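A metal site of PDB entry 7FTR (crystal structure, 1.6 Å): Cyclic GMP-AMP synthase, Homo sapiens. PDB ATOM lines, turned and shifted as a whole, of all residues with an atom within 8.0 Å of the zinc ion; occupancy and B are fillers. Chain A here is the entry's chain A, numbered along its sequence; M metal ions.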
ATOM      1  N   LEU A 227     -20.543  -4.062   3.617  1.00  0.00           N
ATOM      2  CA  LEU A 227     -21.722  -4.895   3.846  1.00  0.00           C
ATOM      3  C   LEU A 227     -22.153  -5.686   2.612  1.00  0.00           C
ATOM      4  O   LEU A 227     -22.676  -6.788   2.746  1.00  0.00           O
ATOM      5  CB  LEU A 227     -22.852  -4.027   4.396  1.00  0.00           C
ATOM      6  CG  LEU A 227     -22.776  -3.872   5.951  1.00  0.00           C
ATOM      7  CD1 LEU A 227     -23.701  -2.791   6.446  1.00  0.00           C
ATOM      8  CD2 LEU A 227     -23.198  -5.150   6.640  1.00  0.00           C
ATOM      9  N   ASN A 229     -19.997  -6.728   0.305  1.00  0.00           N
ATOM     10  CA  ASN A 229     -18.858  -7.558  -0.107  1.00  0.00           C
ATOM     11  C   ASN A 229     -18.159  -7.916   1.186  1.00  0.00           C
ATOM     12  O   ASN A 229     -17.102  -7.367   1.510  1.00  0.00           O
ATOM     13  CB  ASN A 229     -17.972  -6.772  -1.069  1.00  0.00           C
ATOM     14  CG  ASN A 229     -16.961  -7.617  -1.754  1.00  0.00           C
ATOM     15  OD1 ASN A 229     -16.836  -8.823  -1.486  1.00  0.00           O
ATOM     16  ND2 ASN A 229     -16.229  -7.025  -2.683  1.00  0.00           N
ATOM     17  N   HIS A 230     -18.853  -8.698   2.010  1.00  0.00           N
ATOM     18  CA  HIS A 230     -18.541  -8.836   3.447  1.00  0.00           C
ATOM     19  C   HIS A 230     -17.830 -10.094   3.924  1.00  0.00           C
ATOM     20  O   HIS A 230     -17.636 -10.243   5.141  1.00  0.00           O
ATOM     21  CB  HIS A 230     -19.859  -8.762   4.242  1.00  0.00           C
ATOM     22  CG  HIS A 230     -20.815  -9.851   3.816  1.00  0.00           C
ATOM     23  ND1 HIS A 230     -22.003  -9.553   3.208  1.00  0.00           N
ATOM     24  CD2 HIS A 230     -20.702 -11.198   3.921  1.00  0.00           C
ATOM     25  CE1 HIS A 230     -22.572 -10.719   2.936  1.00  0.00           C
ATOM     26  NE2 HIS A 230     -21.826 -11.727   3.373  1.00  0.00           N
ATOM     27  N   GLY A 231     -17.558 -11.018   3.030  1.00  0.00           N
ATOM     28  CA  GLY A 231     -16.956 -12.285   3.443  1.00  0.00           C
ATOM     29  C   GLY A 231     -15.465 -12.320   3.317  1.00  0.00           C
ATOM     30  O   GLY A 231     -14.891 -11.511   2.580  1.00  0.00           O
ATOM     31  N   LYS A 232     -14.820 -13.260   4.011  1.00  0.00           N
ATOM     32  CA  LYS A 232     -13.382 -13.506   3.757  1.00  0.00           C
ATOM     33  C   LYS A 232     -13.338 -14.117   2.328  1.00  0.00           C
ATOM     34  O   LYS A 232     -12.442 -13.790   1.527  1.00  0.00           O
ATOM     35  CB  LYS A 232     -12.832 -14.514   4.792  1.00  0.00           C
ATOM     36  CG  LYS A 232     -11.426 -14.986   4.408  1.00  0.00           C
ATOM     37  CD  LYS A 232     -10.703 -15.750   5.529  1.00  0.00           C
ATOM     38  CE  LYS A 232     -10.269 -14.858   6.677  1.00  0.00           C
ATOM     39  NZ  LYS A 232      -9.521 -13.672   6.217  1.00  0.00           N
ATOM     40  N   SER A 233     -14.311 -15.008   2.002  1.00  0.00           N
ATOM     41  CA  SER A 233     -14.388 -15.615   0.683  1.00  0.00           C
ATOM     42  C   SER A 233     -14.988 -14.586  -0.271  1.00  0.00           C
ATOM     43  O   SER A 233     -15.990 -13.971   0.061  1.00  0.00           O
ATOM     44  CB  SER A 233     -15.282 -16.855   0.686  1.00  0.00           C
ATOM     45  OG  SER A 233     -15.544 -17.222  -0.657  1.00  0.00           O
ATOM     46  N   THR A 235     -16.604 -15.242  -2.751  1.00  0.00           N
ATOM     47  CA  THR A 235     -17.910 -15.792  -3.131  1.00  0.00           C
ATOM     48  C   THR A 235     -18.886 -15.927  -1.945  1.00  0.00           C
ATOM     49  O   THR A 235     -19.917 -16.585  -2.088  1.00  0.00           O
ATOM     50  CB  THR A 235     -17.756 -17.092  -3.930  1.00  0.00           C
ATOM     51  OG1 THR A 235     -16.890 -17.978  -3.230  1.00  0.00           O
ATOM     52  CG2 THR A 235     -17.186 -16.845  -5.333  1.00  0.00           C
ATOM     53  N   CYS A 236     -18.616 -15.260  -0.826  1.00  0.00           N
ATOM     54  CA  CYS A 236     -19.530 -15.331   0.315  1.00  0.00           C
ATOM     55  C   CYS A 236     -20.956 -14.836  -0.103  1.00  0.00           C
ATOM     56  O   CYS A 236     -21.070 -13.830  -0.774  1.00  0.00           O
ATOM     57  CB  CYS A 236     -19.008 -14.546   1.519  1.00  0.00           C
ATOM     58  SG  CYS A 236     -19.892 -14.933   3.050  1.00  0.00           S
ATOM     59  N   CYS A 237     -21.995 -15.644   0.182  1.00  0.00           N
ATOM     60  CA  CYS A 237     -23.407 -15.385  -0.124  1.00  0.00           C
ATOM     61  C   CYS A 237     -23.729 -15.324  -1.667  1.00  0.00           C
ATOM     62  O   CYS A 237     -24.817 -14.912  -2.053  1.00  0.00           O
ATOM     63  CB  CYS A 237     -23.922 -14.163   0.637  1.00  0.00           C
ATOM     64  SG  CYS A 237     -23.745 -14.324   2.435  1.00  0.00           S
ATOM     65  N   GLU A 238     -22.808 -15.804  -2.521  1.00  0.00           N
ATOM     66  CA  GLU A 238     -23.044 -15.860  -3.959  1.00  0.00           C
ATOM     67  C   GLU A 238     -23.536 -17.271  -4.351  1.00  0.00           C
ATOM     68  O   GLU A 238     -24.018 -17.468  -5.467  1.00  0.00           O
ATOM     69  CB  GLU A 238     -21.759 -15.553  -4.738  1.00  0.00           C
ATOM     70  CG  GLU A 238     -21.410 -14.076  -4.831  1.00  0.00           C
ATOM     71  CD  GLU A 238     -20.579 -13.714  -6.045  1.00  0.00           C
ATOM     72  OE1 GLU A 238     -19.970 -14.622  -6.653  1.00  0.00           O
ATOM     73  OE2 GLU A 238     -20.533 -12.518  -6.387  1.00  0.00           O
ATOM     74  N   ASN A 239     -23.375 -18.251  -3.434  1.00  0.00           N
ATOM     75  CA  ASN A 239     -23.798 -19.643  -3.678  1.00  0.00           C
ATOM     76  C   ASN A 239     -24.434 -20.241  -2.431  1.00  0.00           C
ATOM     77  O   ASN A 239     -24.275 -19.701  -1.325  1.00  0.00           O
ATOM     78  CB  ASN A 239     -22.629 -20.497  -4.156  1.00  0.00           C
ATOM     79  CG  ASN A 239     -21.522 -20.649  -3.162  1.00  0.00           C
ATOM     80  OD1 ASN A 239     -21.637 -21.372  -2.176  1.00  0.00           O
ATOM     81  ND2 ASN A 239     -20.427 -19.971  -3.413  1.00  0.00           N
ATOM     82  N   GLU A 242     -22.184 -21.166   0.637  1.00  0.00           N
ATOM     83  CA  GLU A 242     -21.531 -20.071   1.319  1.00  0.00           C
ATOM     84  C   GLU A 242     -22.507 -19.015   1.804  1.00  0.00           C
ATOM     85  O   GLU A 242     -22.144 -17.837   1.810  1.00  0.00           O
ATOM     86  CB  GLU A 242     -20.469 -19.458   0.402  1.00  0.00           C
ATOM     87  CG  GLU A 242     -19.263 -20.348   0.180  1.00  0.00           C
ATOM     88  CD  GLU A 242     -18.200 -19.622  -0.604  1.00  0.00           C
ATOM     89  OE1 GLU A 242     -17.442 -18.830  -0.001  1.00  0.00           O
ATOM     90  OE2 GLU A 242     -18.160 -19.800  -1.830  1.00  0.00           O
ATOM     91  N   LYS A 243     -23.700 -19.427   2.277  1.00  0.00           N
ATOM     92  CA  LYS A 243     -24.688 -18.465   2.800  1.00  0.00           C
ATOM     93  C   LYS A 243     -24.407 -18.123   4.269  1.00  0.00           C
ATOM     94  O   LYS A 243     -24.861 -18.837   5.149  1.00  0.00           O
ATOM     95  CB  LYS A 243     -26.116 -19.009   2.598  1.00  0.00           C
ATOM     96  CG  LYS A 243     -26.580 -18.994   1.134  1.00  0.00           C
ATOM     97  CD  LYS A 243     -27.049 -17.592   0.707  1.00  0.00           C
ATOM     98  CE  LYS A 243     -27.109 -17.415  -0.795  1.00  0.00           C
ATOM     99  NZ  LYS A 243     -27.589 -16.061  -1.164  1.00  0.00           N
ATOM    100  N   CYS A 244     -23.650 -17.041   4.563  1.00  0.00           N
ATOM    101  CA  CYS A 244     -23.349 -16.701   5.965  1.00  0.00           C
ATOM    102  C   CYS A 244     -24.523 -15.973   6.633  1.00  0.00           C
ATOM    103  O   CYS A 244     -25.478 -15.555   5.962  1.00  0.00           O
ATOM    104  CB  CYS A 244     -22.045 -15.905   6.081  1.00  0.00           C
ATOM    105  SG  CYS A 244     -22.227 -14.131   5.731  1.00  0.00           S
ATOM    106  N   CYS A 245     -24.475 -15.858   7.960  1.00  0.00           N
ATOM    107  CA  CYS A 245     -25.531 -15.194   8.707  1.00  0.00           C
ATOM    108  C   CYS A 245     -25.110 -13.789   9.192  1.00  0.00           C
ATOM    109  O   CYS A 245     -25.770 -13.265  10.080  1.00  0.00           O
ATOM    110  CB  CYS A 245     -26.010 -16.064   9.871  1.00  0.00           C
ATOM    111  SG  CYS A 245     -24.779 -16.276  11.189  1.00  0.00           S
ATOM    112  N   ARG A 246     -24.091 -13.157   8.593  1.00  0.00           N
ATOM    113  CA  ARG A 246     -23.680 -11.797   9.035  1.00  0.00           C
ATOM    114  C   ARG A 246     -24.800 -10.785   8.911  1.00  0.00           C
ATOM    115  O   ARG A 246     -25.077 -10.061   9.876  1.00  0.00           O
ATOM    116  CB  ARG A 246     -22.471 -11.280   8.202  1.00  0.00           C
ATOM    117  CG  ARG A 246     -21.147 -11.984   8.537  1.00  0.00           C
ATOM    118  CD  ARG A 246     -20.036 -11.329   7.768  1.00  0.00           C
ATOM    119  NE  ARG A 246     -18.720 -11.891   8.029  1.00  0.00           N
ATOM    120  CZ  ARG A 246     -18.201 -12.906   7.341  1.00  0.00           C
ATOM    121  NH1 ARG A 246     -16.940 -13.271   7.544  1.00  0.00           N
ATOM    122  NH2 ARG A 246     -18.933 -13.547   6.423  1.00  0.00           N
ATOM    123  N   LYS A 247     -25.436 -10.716   7.736  1.00  0.00           N
ATOM    124  CA  LYS A 247     -26.505  -9.692   7.573  1.00  0.00           C
ATOM    125  C   LYS A 247     -27.690 -10.004   8.433  1.00  0.00           C
ATOM    126  O   LYS A 247     -28.329  -9.075   8.952  1.00  0.00           O
ATOM    127  CB  LYS A 247     -26.896  -9.535   6.103  1.00  0.00           C
ATOM    128  CG  LYS A 247     -25.804  -8.895   5.285  1.00  0.00           C
ATOM    129  CD  LYS A 247     -26.390  -8.374   3.919  1.00  0.00           C
ATOM    130  CE  LYS A 247     -25.346  -7.538   3.236  1.00  0.00           C
ATOM    131  NZ  LYS A 247     -25.762  -7.020   1.916  1.00  0.00           N
ATOM    132  N   ASP A 292     -15.468 -16.832   7.621  1.00  0.00           N
ATOM    133  CA  ASP A 292     -16.849 -17.103   7.209  1.00  0.00           C
ATOM    134  C   ASP A 292     -17.420 -18.300   8.001  1.00  0.00           C
ATOM    135  O   ASP A 292     -18.624 -18.331   8.275  1.00  0.00           O
ATOM    136  CB  ASP A 292     -16.927 -17.364   5.709  1.00  0.00           C
ATOM    137  CG  ASP A 292     -16.515 -16.183   4.857  1.00  0.00           C
ATOM    138  OD1 ASP A 292     -16.589 -15.042   5.333  1.00  0.00           O
ATOM    139  OD2 ASP A 292     -16.156 -16.398   3.684  1.00  0.00           O
ATOM    140  N   TRP A 295     -19.599 -17.559  10.962  1.00  0.00           N
ATOM    141  CA  TRP A 295     -20.905 -16.994  10.621  1.00  0.00           C
ATOM    142  C   TRP A 295     -21.716 -18.003   9.838  1.00  0.00           C
ATOM    143  O   TRP A 295     -22.479 -17.633   8.956  1.00  0.00           O
ATOM    144  CB  TRP A 295     -20.781 -15.663   9.848  1.00  0.00           C
ATOM    145  CG  TRP A 295     -20.020 -14.614  10.598  1.00  0.00           C
ATOM    146  CD1 TRP A 295     -18.674 -14.381  10.546  1.00  0.00           C
ATOM    147  CD2 TRP A 295     -20.553 -13.693  11.539  1.00  0.00           C
ATOM    148  NE1 TRP A 295     -18.335 -13.362  11.413  1.00  0.00           N
ATOM    149  CE2 TRP A 295     -19.482 -12.878  11.983  1.00  0.00           C
ATOM    150  CE3 TRP A 295     -21.854 -13.441  12.026  1.00  0.00           C
ATOM    151  CZ2 TRP A 295     -19.672 -11.808  12.880  1.00  0.00           C
ATOM    152  CZ3 TRP A 295     -22.034 -12.406  12.941  1.00  0.00           C
ATOM    153  CH2 TRP A 295     -20.953 -11.597  13.355  1.00  0.00           C
HETATM  154 ZN    ZN M   1     -21.906 -13.833   3.377  1.00  0.00          ZN
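Within 4 Å of the zinc ion: His 230, Cys 236, Cys 237 and Cys 244.
The zinc ion is bound by a ring nitrogen (NE2) of His 230 (2.1 Å), the side-chain sulfur (SG) of Cys 237 (2.1 Å), the side-chain sulfur (SG) of Cys 236 (2.3 Å) and the side-chain sulfur (SG) of Cys 244 (2.4 Å).
A ring nitrogen (ND1) of His 230 sits at hydrogen-bond distance from the backbone carbonyl oxygen (O) of Leu 227, 2.9 Å away. The guanidinium group (NH2) of Arg 246 lies close to the side-chain sulfur (SG) of Cys 236. NZ of Lys 243 lies within hydrogen-bond range of O of Cys 237 (3.1 Å). N of Cys 237 lies within hydrogen-bond range of O of Glu 242, at 2.7 Å. The side-chain sulfur (SG) of Cys 244 lies close to the guanidinium group (NH2) of Arg 246, at 3.4 Å. NE of Arg 246 lies within hydrogen-bond range of O of His 230 (3.5 Å).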
